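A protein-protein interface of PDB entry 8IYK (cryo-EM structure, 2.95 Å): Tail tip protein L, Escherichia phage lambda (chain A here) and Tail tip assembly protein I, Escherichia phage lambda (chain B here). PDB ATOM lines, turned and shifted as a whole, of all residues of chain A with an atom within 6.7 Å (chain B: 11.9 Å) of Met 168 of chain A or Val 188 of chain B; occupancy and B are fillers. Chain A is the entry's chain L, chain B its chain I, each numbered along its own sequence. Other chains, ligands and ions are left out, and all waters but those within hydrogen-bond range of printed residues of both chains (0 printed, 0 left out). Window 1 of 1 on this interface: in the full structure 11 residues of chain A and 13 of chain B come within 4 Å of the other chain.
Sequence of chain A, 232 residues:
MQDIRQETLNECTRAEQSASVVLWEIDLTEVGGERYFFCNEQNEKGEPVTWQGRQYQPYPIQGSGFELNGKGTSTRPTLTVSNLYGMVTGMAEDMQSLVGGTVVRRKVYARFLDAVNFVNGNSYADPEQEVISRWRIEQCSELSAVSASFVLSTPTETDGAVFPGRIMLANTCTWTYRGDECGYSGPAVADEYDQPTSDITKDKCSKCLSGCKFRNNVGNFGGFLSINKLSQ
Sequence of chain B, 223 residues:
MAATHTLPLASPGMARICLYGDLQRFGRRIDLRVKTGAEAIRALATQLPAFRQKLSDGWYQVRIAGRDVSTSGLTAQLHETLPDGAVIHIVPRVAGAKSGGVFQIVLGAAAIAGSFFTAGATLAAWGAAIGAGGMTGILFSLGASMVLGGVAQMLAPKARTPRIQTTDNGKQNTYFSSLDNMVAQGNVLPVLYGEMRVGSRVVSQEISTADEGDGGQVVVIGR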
ATOM      1  N   VAL A 162      -9.073  -6.317 -26.964  1.00  0.00           N
ATOM      2  CA  VAL A 162      -8.817  -7.088 -25.756  1.00  0.00           C
ATOM      3  C   VAL A 162      -9.287  -6.270 -24.562  1.00  0.00           C
ATOM      4  O   VAL A 162      -9.437  -5.049 -24.634  1.00  0.00           O
ATOM      5  CB  VAL A 162      -7.328  -7.460 -25.604  1.00  0.00           C
ATOM      6  CG1 VAL A 162      -6.948  -8.538 -26.600  1.00  0.00           C
ATOM      7  CG2 VAL A 162      -6.461  -6.231 -25.793  1.00  0.00           C
ATOM      8  N   PHE A 163      -9.522  -6.964 -23.447  1.00  0.00           N
ATOM      9  CA  PHE A 163      -9.983  -6.298 -22.246  1.00  0.00           C
ATOM     10  C   PHE A 163      -9.484  -7.051 -21.021  1.00  0.00           C
ATOM     11  O   PHE A 163      -9.702  -8.269 -20.930  1.00  0.00           O
ATOM     12  CB  PHE A 163     -11.507  -6.199 -22.210  1.00  0.00           C
ATOM     13  CG  PHE A 163     -12.036  -5.340 -21.099  1.00  0.00           C
ATOM     14  CD1 PHE A 163     -12.120  -3.970 -21.248  1.00  0.00           C
ATOM     15  CD2 PHE A 163     -12.451  -5.904 -19.906  1.00  0.00           C
ATOM     16  CE1 PHE A 163     -12.605  -3.179 -20.229  1.00  0.00           C
ATOM     17  CE2 PHE A 163     -12.936  -5.116 -18.883  1.00  0.00           C
ATOM     18  CZ  PHE A 163     -13.013  -3.753 -19.046  1.00  0.00           C
ATOM     19  N   PRO A 164      -8.822  -6.375 -20.074  1.00  0.00           N
ATOM     20  CA  PRO A 164      -8.429  -4.957 -20.079  1.00  0.00           C
ATOM     21  C   PRO A 164      -7.256  -4.710 -21.022  1.00  0.00           C
ATOM     22  O   PRO A 164      -6.461  -5.608 -21.272  1.00  0.00           O
ATOM     23  CB  PRO A 164      -8.055  -4.688 -18.610  1.00  0.00           C
ATOM     24  CG  PRO A 164      -8.588  -5.860 -17.826  1.00  0.00           C
ATOM     25  CD  PRO A 164      -8.525  -7.006 -18.781  1.00  0.00           C
ATOM     26  N   GLY A 165      -7.114  -3.499 -21.555  1.00  0.00           N
ATOM     27  CA  GLY A 165      -6.114  -3.243 -22.573  1.00  0.00           C
ATOM     28  C   GLY A 165      -4.846  -2.573 -22.087  1.00  0.00           C
ATOM     29  O   GLY A 165      -3.781  -2.757 -22.686  1.00  0.00           O
ATOM     30  N   ARG A 166      -4.937  -1.793 -21.014  1.00  0.00           N
ATOM     31  CA  ARG A 166      -3.767  -1.086 -20.508  1.00  0.00           C
ATOM     32  C   ARG A 166      -2.764  -2.080 -19.938  1.00  0.00           C
ATOM     33  O   ARG A 166      -3.124  -2.948 -19.140  1.00  0.00           O
ATOM     34  CB  ARG A 166      -4.176  -0.073 -19.444  1.00  0.00           C
ATOM     35  CG  ARG A 166      -3.192   1.064 -19.273  1.00  0.00           C
ATOM     36  CD  ARG A 166      -3.678   2.058 -18.242  1.00  0.00           C
ATOM     37  NE  ARG A 166      -2.593   2.530 -17.392  1.00  0.00           N
ATOM     38  CZ  ARG A 166      -2.730   2.867 -16.118  1.00  0.00           C
ATOM     39  NH1 ARG A 166      -3.895   2.774 -15.500  1.00  0.00           N
ATOM     40  NH2 ARG A 166      -1.671   3.313 -15.450  1.00  0.00           N
ATOM     41  N   ILE A 167      -1.502  -1.943 -20.338  1.00  0.00           N
ATOM     42  CA  ILE A 167      -0.465  -2.915 -20.018  1.00  0.00           C
ATOM     43  C   ILE A 167       0.517  -2.300 -19.029  1.00  0.00           C
ATOM     44  O   ILE A 167       0.752  -1.086 -19.025  1.00  0.00           O
ATOM     45  CB  ILE A 167       0.251  -3.399 -21.298  1.00  0.00           C
ATOM     46  CG1 ILE A 167       1.189  -4.568 -20.994  1.00  0.00           C
ATOM     47  CG2 ILE A 167       0.995  -2.254 -21.962  1.00  0.00           C
ATOM     48  CD1 ILE A 167       2.037  -4.992 -22.169  1.00  0.00           C
ATOM     49  N   MET A 168       1.084  -3.152 -18.175  1.00  0.00           N
ATOM     50  CA  MET A 168       2.041  -2.745 -17.152  1.00  0.00           C
ATOM     51  C   MET A 168       3.449  -2.927 -17.705  1.00  0.00           C
ATOM     52  O   MET A 168       3.908  -4.057 -17.890  1.00  0.00           O
ATOM     53  CB  MET A 168       1.844  -3.563 -15.878  1.00  0.00           C
ATOM     54  CG  MET A 168       0.416  -3.583 -15.360  1.00  0.00           C
ATOM     55  SD  MET A 168       0.305  -3.787 -13.572  1.00  0.00           S
ATOM     56  CE  MET A 168       1.291  -2.411 -12.999  1.00  0.00           C
ATOM     57  N   LEU A 169       4.138  -1.817 -17.957  1.00  0.00           N
ATOM     58  CA  LEU A 169       5.475  -1.843 -18.530  1.00  0.00           C
ATOM     59  C   LEU A 169       6.407  -0.929 -17.751  1.00  0.00           C
ATOM     60  O   LEU A 169       5.975   0.033 -17.114  1.00  0.00           O
ATOM     61  CB  LEU A 169       5.476  -1.407 -19.998  1.00  0.00           C
ATOM     62  CG  LEU A 169       4.817  -2.318 -21.028  1.00  0.00           C
ATOM     63  CD1 LEU A 169       4.562  -1.541 -22.301  1.00  0.00           C
ATOM     64  CD2 LEU A 169       5.697  -3.517 -21.302  1.00  0.00           C
ATOM     65  N   ALA A 170       7.694  -1.246 -17.816  1.00  0.00           N
ATOM     66  CA  ALA A 170       8.749  -0.365 -17.349  1.00  0.00           C
ATOM     67  C   ALA A 170       9.509   0.188 -18.548  1.00  0.00           C
ATOM     68  O   ALA A 170       9.529  -0.418 -19.623  1.00  0.00           O
ATOM     69  CB  ALA A 170       9.713  -1.094 -16.411  1.00  0.00           C
ATOM     70  N   THR A 174       2.751   4.218 -21.809  1.00  0.00           N
ATOM     71  CA  THR A 174       1.622   3.752 -22.603  1.00  0.00           C
ATOM     72  C   THR A 174       0.606   4.848 -22.893  1.00  0.00           C
ATOM     73  O   THR A 174      -0.390   4.582 -23.572  1.00  0.00           O
ATOM     74  CB  THR A 174       0.924   2.587 -21.895  1.00  0.00           C
ATOM     75  OG1 THR A 174       0.184   3.083 -20.774  1.00  0.00           O
ATOM     76  CG2 THR A 174       1.946   1.576 -21.410  1.00  0.00           C
ATOM     77  N   GLY A 222       3.524   7.099 -17.727  1.00  0.00           N
ATOM     78  CA  GLY A 222       2.634   5.963 -17.822  1.00  0.00           C
ATOM     79  C   GLY A 222       3.241   4.620 -17.505  1.00  0.00           C
ATOM     80  O   GLY A 222       2.521   3.620 -17.476  1.00  0.00           O
ATOM     81  N   GLY A 223       4.551   4.564 -17.265  1.00  0.00           N
ATOM     82  CA  GLY A 223       5.217   3.334 -16.902  1.00  0.00           C
ATOM     83  C   GLY A 223       5.318   3.161 -15.394  1.00  0.00           C
ATOM     84  O   GLY A 223       4.898   4.002 -14.604  1.00  0.00           O
ATOM     85  N   PHE A 224       5.893   2.028 -15.006  1.00  0.00           N
ATOM     86  CA  PHE A 224       6.101   1.676 -13.604  1.00  0.00           C
ATOM     87  C   PHE A 224       7.590   1.404 -13.433  1.00  0.00           C
ATOM     88  O   PHE A 224       8.079   0.338 -13.819  1.00  0.00           O
ATOM     89  CB  PHE A 224       5.253   0.469 -13.212  1.00  0.00           C
ATOM     90  CG  PHE A 224       3.792   0.628 -13.526  1.00  0.00           C
ATOM     91  CD1 PHE A 224       3.307   0.356 -14.793  1.00  0.00           C
ATOM     92  CD2 PHE A 224       2.903   1.058 -12.557  1.00  0.00           C
ATOM     93  CE1 PHE A 224       1.968   0.507 -15.086  1.00  0.00           C
ATOM     94  CE2 PHE A 224       1.561   1.209 -12.846  1.00  0.00           C
ATOM     95  CZ  PHE A 224       1.094   0.934 -14.111  1.00  0.00           C
ATOM     96  N   ILE A 227       9.254  -2.353 -11.830  1.00  0.00           N
ATOM     97  CA  ILE A 227       8.824  -3.724 -12.071  1.00  0.00           C
ATOM     98  C   ILE A 227       9.854  -4.566 -12.800  1.00  0.00           C
ATOM     99  O   ILE A 227       9.696  -5.790 -12.871  1.00  0.00           O
ATOM    100  CB  ILE A 227       7.502  -3.726 -12.864  1.00  0.00           C
ATOM    101  CG1 ILE A 227       7.748  -3.246 -14.293  1.00  0.00           C
ATOM    102  CG2 ILE A 227       6.475  -2.851 -12.176  1.00  0.00           C
ATOM    103  CD1 ILE A 227       6.573  -3.439 -15.219  1.00  0.00           C
ATOM    104  N   TYR B 175     -12.644 -17.024 -13.988  1.00  0.00           N
ATOM    105  CA  TYR B 175     -12.102 -15.966 -14.825  1.00  0.00           C
ATOM    106  C   TYR B 175     -12.383 -14.579 -14.269  1.00  0.00           C
ATOM    107  O   TYR B 175     -12.140 -13.588 -14.962  1.00  0.00           O
ATOM    108  CB  TYR B 175     -12.658 -16.073 -16.246  1.00  0.00           C
ATOM    109  CG  TYR B 175     -11.721 -16.732 -17.227  1.00  0.00           C
ATOM    110  CD1 TYR B 175     -10.365 -16.441 -17.221  1.00  0.00           C
ATOM    111  CD2 TYR B 175     -12.194 -17.627 -18.174  1.00  0.00           C
ATOM    112  CE1 TYR B 175      -9.506 -17.035 -18.118  1.00  0.00           C
ATOM    113  CE2 TYR B 175     -11.342 -18.224 -19.078  1.00  0.00           C
ATOM    114  CZ  TYR B 175      -9.998 -17.924 -19.045  1.00  0.00           C
ATOM    115  OH  TYR B 175      -9.140 -18.514 -19.943  1.00  0.00           O
ATOM    116  N   SER B 178      -9.172 -13.351  -8.192  1.00  0.00           N
ATOM    117  CA  SER B 178      -7.807 -13.779  -7.920  1.00  0.00           C
ATOM    118  C   SER B 178      -7.432 -13.325  -6.520  1.00  0.00           C
ATOM    119  O   SER B 178      -7.664 -12.168  -6.160  1.00  0.00           O
ATOM    120  CB  SER B 178      -6.830 -13.202  -8.949  1.00  0.00           C
ATOM    121  OG  SER B 178      -5.530 -13.737  -8.773  1.00  0.00           O
ATOM    122  N   ASP B 180      -4.162 -13.711  -5.377  1.00  0.00           N
ATOM    123  CA  ASP B 180      -2.716 -13.837  -5.452  1.00  0.00           C
ATOM    124  C   ASP B 180      -2.090 -12.480  -5.736  1.00  0.00           C
ATOM    125  O   ASP B 180      -2.726 -11.580  -6.293  1.00  0.00           O
ATOM    126  CB  ASP B 180      -2.299 -14.830  -6.543  1.00  0.00           C
ATOM    127  CG  ASP B 180      -3.227 -16.026  -6.633  1.00  0.00           C
ATOM    128  OD1 ASP B 180      -3.712 -16.488  -5.580  1.00  0.00           O
ATOM    129  OD2 ASP B 180      -3.475 -16.502  -7.760  1.00  0.00           O
ATOM    130  N   ASN B 181      -0.825 -12.343  -5.345  1.00  0.00           N
ATOM    131  CA  ASN B 181      -0.029 -11.151  -5.636  1.00  0.00           C
ATOM    132  C   ASN B 181       0.849 -11.487  -6.836  1.00  0.00           C
ATOM    133  O   ASN B 181       1.992 -11.920  -6.695  1.00  0.00           O
ATOM    134  CB  ASN B 181       0.790 -10.733  -4.421  1.00  0.00           C
ATOM    135  CG  ASN B 181      -0.074 -10.261  -3.269  1.00  0.00           C
ATOM    136  OD1 ASN B 181      -0.774  -9.258  -3.374  1.00  0.00           O
ATOM    137  ND2 ASN B 181      -0.027 -10.988  -2.160  1.00  0.00           N
ATOM    138  N   MET B 182       0.299 -11.282  -8.030  1.00  0.00           N
ATOM    139  CA  MET B 182       0.918 -11.742  -9.262  1.00  0.00           C
ATOM    140  C   MET B 182       2.036 -10.800  -9.705  1.00  0.00           C
ATOM    141  O   MET B 182       2.206  -9.695  -9.188  1.00  0.00           O
ATOM    142  CB  MET B 182      -0.130 -11.870 -10.364  1.00  0.00           C
ATOM    143  CG  MET B 182      -1.366 -12.648  -9.953  1.00  0.00           C
ATOM    144  SD  MET B 182      -2.840 -12.140 -10.855  1.00  0.00           S
ATOM    145  CE  MET B 182      -3.125 -10.517 -10.156  1.00  0.00           C
ATOM    146  N   VAL B 183       2.810 -11.264 -10.688  1.00  0.00           N
ATOM    147  CA  VAL B 183       3.861 -10.447 -11.279  1.00  0.00           C
ATOM    148  C   VAL B 183       3.230  -9.367 -12.148  1.00  0.00           C
ATOM    149  O   VAL B 183       2.240  -9.607 -12.852  1.00  0.00           O
ATOM    150  CB  VAL B 183       4.828 -11.336 -12.082  1.00  0.00           C
ATOM    151  CG1 VAL B 183       5.682 -10.510 -13.027  1.00  0.00           C
ATOM    152  CG2 VAL B 183       5.704 -12.146 -11.141  1.00  0.00           C
ATOM    153  N   ALA B 184       3.799  -8.165 -12.102  1.00  0.00           N
ATOM    154  CA  ALA B 184       3.212  -6.985 -12.727  1.00  0.00           C
ATOM    155  C   ALA B 184       4.058  -6.454 -13.880  1.00  0.00           C
ATOM    156  O   ALA B 184       4.268  -5.248 -14.004  1.00  0.00           O
ATOM    157  CB  ALA B 184       2.995  -5.886 -11.692  1.00  0.00           C
ATOM    158  N   GLN B 185       4.554  -7.342 -14.737  1.00  0.00           N
ATOM    159  CA  GLN B 185       5.338  -6.952 -15.903  1.00  0.00           C
ATOM    160  C   GLN B 185       4.657  -7.489 -17.154  1.00  0.00           C
ATOM    161  O   GLN B 185       4.528  -8.706 -17.319  1.00  0.00           O
ATOM    162  CB  GLN B 185       6.772  -7.474 -15.799  1.00  0.00           C
ATOM    163  CG  GLN B 185       7.480  -7.641 -17.131  1.00  0.00           C
ATOM    164  CD  GLN B 185       8.475  -6.534 -17.411  1.00  0.00           C
ATOM    165  OE1 GLN B 185       9.375  -6.281 -16.613  1.00  0.00           O
ATOM    166  NE2 GLN B 185       8.320  -5.872 -18.549  1.00  0.00           N
ATOM    167  N   GLY B 186       4.220  -6.582 -18.027  1.00  0.00           N
ATOM    168  CA  GLY B 186       3.577  -6.961 -19.273  1.00  0.00           C
ATOM    169  C   GLY B 186       2.349  -7.825 -19.077  1.00  0.00           C
ATOM    170  O   GLY B 186       2.203  -8.855 -19.741  1.00  0.00           O
ATOM    171  N   ASN B 187       1.456  -7.423 -18.171  1.00  0.00           N
ATOM    172  CA  ASN B 187       0.447  -8.333 -17.659  1.00  0.00           C
ATOM    173  C   ASN B 187      -0.970  -7.774 -17.603  1.00  0.00           C
ATOM    174  O   ASN B 187      -1.868  -8.501 -17.171  1.00  0.00           O
ATOM    175  CB  ASN B 187       0.845  -8.797 -16.253  1.00  0.00           C
ATOM    176  CG  ASN B 187       1.276 -10.236 -16.221  1.00  0.00           C
ATOM    177  OD1 ASN B 187       0.838 -11.049 -17.032  1.00  0.00           O
ATOM    178  ND2 ASN B 187       2.155 -10.561 -15.286  1.00  0.00           N
ATOM    179  N   VAL B 188      -1.183  -6.520 -18.020  1.00  0.00           N
ATOM    180  CA  VAL B 188      -2.408  -5.713 -17.915  1.00  0.00           C
ATOM    181  C   VAL B 188      -2.832  -5.610 -16.452  1.00  0.00           C
ATOM    182  O   VAL B 188      -2.722  -6.575 -15.690  1.00  0.00           O
ATOM    183  CB  VAL B 188      -3.571  -6.204 -18.812  1.00  0.00           C
ATOM    184  CG1 VAL B 188      -3.159  -6.223 -20.283  1.00  0.00           C
ATOM    185  CG2 VAL B 188      -4.239  -7.492 -18.348  1.00  0.00           C
ATOM    186  N   LEU B 189      -3.356  -4.401 -16.199  1.00  0.00           N
ATOM    187  CA  LEU B 189      -3.783  -3.990 -14.854  1.00  0.00           C
ATOM    188  C   LEU B 189      -5.197  -4.471 -14.643  1.00  0.00           C
ATOM    189  O   LEU B 189      -6.030  -4.170 -15.461  1.00  0.00           O
ATOM    190  CB  LEU B 189      -3.712  -2.459 -14.837  1.00  0.00           C
ATOM    191  CG  LEU B 189      -4.202  -1.756 -13.577  1.00  0.00           C
ATOM    192  CD1 LEU B 189      -3.338  -2.116 -12.390  1.00  0.00           C
ATOM    193  CD2 LEU B 189      -4.198  -0.259 -13.780  1.00  0.00           C
ATOM    194  N   PRO B 190      -5.500  -5.176 -13.560  1.00  0.00           N
ATOM    195  CA  PRO B 190      -6.803  -5.730 -13.441  1.00  0.00           C
ATOM    196  C   PRO B 190      -7.930  -4.714 -13.340  1.00  0.00           C
ATOM    197  O   PRO B 190      -7.611  -3.638 -13.053  1.00  0.00           O
ATOM    198  CB  PRO B 190      -6.576  -6.513 -12.163  1.00  0.00           C
ATOM    199  CG  PRO B 190      -5.541  -5.776 -11.403  1.00  0.00           C
ATOM    200  CD  PRO B 190      -4.560  -5.482 -12.498  1.00  0.00           C
ATOM    201  N   VAL B 191      -9.154  -5.045 -13.730  1.00  0.00           N
ATOM    202  CA  VAL B 191     -10.362  -4.246 -13.523  1.00  0.00           C
ATOM    203  C   VAL B 191     -11.166  -4.882 -12.396  1.00  0.00           C
ATOM    204  O   VAL B 191     -11.361  -6.101 -12.379  1.00  0.00           O
ATOM    205  CB  VAL B 191     -11.237  -4.131 -14.789  1.00  0.00           C
ATOM    206  CG1 VAL B 191     -12.506  -3.374 -14.471  1.00  0.00           C
ATOM    207  CG2 VAL B 191     -10.501  -3.424 -15.910  1.00  0.00           C
ATOM    208  N   LEU B 192     -11.637  -4.060 -11.459  1.00  0.00           N
ATOM    209  CA  LEU B 192     -12.458  -4.514 -10.342  1.00  0.00           C
ATOM    210  C   LEU B 192     -13.835  -3.870 -10.439  1.00  0.00           C
ATOM    211  O   LEU B 192     -13.941  -2.646 -10.552  1.00  0.00           O
ATOM    212  CB  LEU B 192     -11.801  -4.169  -9.003  1.00  0.00           C
ATOM    213  CG  LEU B 192     -12.662  -4.241  -7.739  1.00  0.00           C
ATOM    214  CD1 LEU B 192     -13.317  -5.598  -7.609  1.00  0.00           C
ATOM    215  CD2 LEU B 192     -11.832  -3.937  -6.508  1.00  0.00           C
ATOM    216  N   GLY B 199      -6.425  -9.851  -4.858  1.00  0.00           N
ATOM    217  CA  GLY B 199      -4.988  -9.884  -4.702  1.00  0.00           C
ATOM    218  C   GLY B 199      -4.408  -8.566  -5.161  1.00  0.00           C
ATOM    219  O   GLY B 199      -4.925  -7.510  -4.787  1.00  0.00           O
ATOM    220  N   SER B 200      -3.361  -8.601  -5.983  1.00  0.00           N
ATOM    221  CA  SER B 200      -2.756  -7.373  -6.485  1.00  0.00           C
ATOM    222  C   SER B 200      -1.689  -7.726  -7.511  1.00  0.00           C
ATOM    223  O   SER B 200      -1.303  -8.887  -7.669  1.00  0.00           O
ATOM    224  CB  SER B 200      -2.140  -6.539  -5.365  1.00  0.00           C
ATOM    225  OG  SER B 200      -1.620  -7.367  -4.340  1.00  0.00           O
ATOM    226  N   ARG B 201      -1.220  -6.698  -8.209  1.00  0.00           N
ATOM    227  CA  ARG B 201      -0.040  -6.768  -9.064  1.00  0.00           C
ATOM    228  C   ARG B 201       1.044  -5.965  -8.356  1.00  0.00           C
ATOM    229  O   ARG B 201       1.009  -4.732  -8.351  1.00  0.00           O
ATOM    230  CB  ARG B 201      -0.330  -6.215 -10.454  1.00  0.00           C
ATOM    231  CG  ARG B 201      -1.449  -6.916 -11.196  1.00  0.00           C
ATOM    232  CD  ARG B 201      -1.076  -7.143 -12.648  1.00  0.00           C
ATOM    233  NE  ARG B 201      -2.054  -7.969 -13.343  1.00  0.00           N
ATOM    234  CZ  ARG B 201      -1.838  -9.218 -13.730  1.00  0.00           C
ATOM    235  NH1 ARG B 201      -0.686  -9.825 -13.498  1.00  0.00           N
ATOM    236  NH2 ARG B 201      -2.803  -9.875 -14.367  1.00  0.00           N
ATOM    237  N   VAL B 202       2.001  -6.666  -7.750  1.00  0.00           N
ATOM    238  CA  VAL B 202       2.998  -6.008  -6.912  1.00  0.00           C
ATOM    239  C   VAL B 202       3.853  -5.091  -7.775  1.00  0.00           C
ATOM    240  O   VAL B 202       4.508  -5.538  -8.722  1.00  0.00           O
ATOM    241  CB  VAL B 202       3.858  -7.041  -6.174  1.00  0.00           C
ATOM    242  CG1 VAL B 202       4.532  -6.404  -4.971  1.00  0.00           C
ATOM    243  CG2 VAL B 202       3.009  -8.218  -5.747  1.00  0.00           C
ATOM    244  N   VAL B 203       3.851  -3.803  -7.445  1.00  0.00           N
ATOM    245  CA  VAL B 203       4.630  -2.822  -8.191  1.00  0.00           C
ATOM    246  C   VAL B 203       6.006  -2.620  -7.570  1.00  0.00           C
ATOM    247  O   VAL B 203       7.013  -2.568  -8.280  1.00  0.00           O
ATOM    248  CB  VAL B 203       3.847  -1.496  -8.284  1.00  0.00           C
ATOM    249  CG1 VAL B 203       4.796  -0.313  -8.385  1.00  0.00           C
ATOM    250  CG2 VAL B 203       2.902  -1.525  -9.470  1.00  0.00           C
ATOM    251  N   SER B 204       6.071  -2.513  -6.247  1.00  0.00           N
ATOM    252  CA  SER B 204       7.331  -2.371  -5.537  1.00  0.00           C
ATOM    253  C   SER B 204       7.284  -3.212  -4.272  1.00  0.00           C
ATOM    254  O   SER B 204       6.256  -3.263  -3.593  1.00  0.00           O
ATOM    255  CB  SER B 204       7.618  -0.908  -5.185  1.00  0.00           C
ATOM    256  OG  SER B 204       7.434  -0.673  -3.802  1.00  0.00           O
ATOM    257  N   GLN B 205       8.394  -3.878  -3.966  1.00  0.00           N
ATOM    258  CA  GLN B 205       8.504  -4.658  -2.737  1.00  0.00           C
ATOM    259  C   GLN B 205       9.936  -4.530  -2.239  1.00  0.00           C
ATOM    260  O   GLN B 205      10.859  -5.063  -2.860  1.00  0.00           O
ATOM    261  CB  GLN B 205       8.124  -6.117  -2.965  1.00  0.00           C
ATOM    262  CG  GLN B 205       7.978  -6.918  -1.685  1.00  0.00           C
ATOM    263  CD  GLN B 205       7.321  -8.263  -1.913  1.00  0.00           C
ATOM    264  OE1 GLN B 205       6.788  -8.530  -2.987  1.00  0.00           O
ATOM    265  NE2 GLN B 205       7.356  -9.118  -0.899  1.00  0.00           N
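Pro 164 of chain A touches Val 188 of chain B. Leu 189 of chain B touches Pro 164 of chain A (O to CB, 3.8 Å). Pro 164 of chain A touches Val 191 of chain B. Arg 166 of chain A touches Val 188 of chain B. CG1 of Ile 167 of chain A touches CA of Gly 186 of chain B (3.8 Å). Met 168 of chain A touches Ala 184 of chain B. Gln 185 of chain B touches Met 168 of chain A. Leu 189 of chain B touches Met 168 of chain A (N to CG, 3.9 Å). SD of Met 168 of chain A touches CD of Arg 201 of chain B, at 3.7 Å. O of Val 203 of chain B touches CG2 of Ile 227 of chain A (3.9 Å).
Of the printed residues of chain B, Met 168 of chain A touches Ala 184 (3.5 Å), Gln 185 (3.6 Å), Gly 186 (2.5 Å), Val 188 (3.98 Å), Leu 189 (3.9 Å), Arg 201 (3.7 Å) and Val 203 (3.98 Å). Printed residues of chain A within 4 Å of Val 188 of chain B: Pro 164, Arg 166 and Met 168. No residue of chain B comes within 4 Å of Gly 165 of chain A. No residue of chain B comes within 4 Å of Leu 169 of chain A. No residue of chain B comes within 4 Å of Ala 170 of chain A. No residue of chain B comes within 4 Å of Gly 223 of chain A. Of the printed residues of chain A, Leu 189 of chain B touches Pro 164 (3.8 Å), Arg 166 (3.3 Å) and Met 168 (3.9 Å). Of the printed residues of chain A, Gln 185 of chain B touches Met 168 (3.6 Å) and Ile 227 (3.8 Å). Of the printed residues of chain B, Ile 227 of chain A touches Ala 184 (3.2 Å), Gln 185 (3.8 Å) and Val 203 (3.9 Å). Printed residues of chain A within 4 Å of Val 191 of chain B: Pro 164. Ser 200 of chain B touches none of the printed residues of chain A. Ser 204 of chain B touches none of the printed residues of chain A. The nearest printed residue of chain B that does not touch Met 168 of chain A is Asn 187 of chain B (4.2 Å).
Of the 22 printed residues of chain B, 8 touch a printed residue of chain A. Printed residues of chain A that touch a printed residue of chain B: Pro 164, Arg 166, Ile 167, Met 168 and Ile 227. Among the printed residues, no Asp or Glu carboxylate lies within 4 Å of a Lys or Arg side-chain nitrogen of the other chain.
The guanidinium group (NH1) of Arg 201 of chain B sits at hydrogen-bond distance from the backbone carbonyl oxygen (O) of Val 183 of chain B. The backbone carbonyl oxygen (O) of Asn 187 of chain B sits at hydrogen-bond distance from the guanidinium group (NH2) of Arg 201 of chain B, at 3.3 Å. O of Val 188 of chain B sits at hydrogen-bond distance from NE of Arg 201 of chain B (2.8 Å).
The backbone carbonyl oxygen (O) of Arg 166 of chain A sits at hydrogen-bond distance from the backbone NH (N) of Leu 189 of chain B (3.3 Å). The backbone NH (N) of Gly 186 of chain B lies within hydrogen-bond range of the backbone carbonyl oxygen (O) of Met 168 of chain A, 2.5 Å away.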
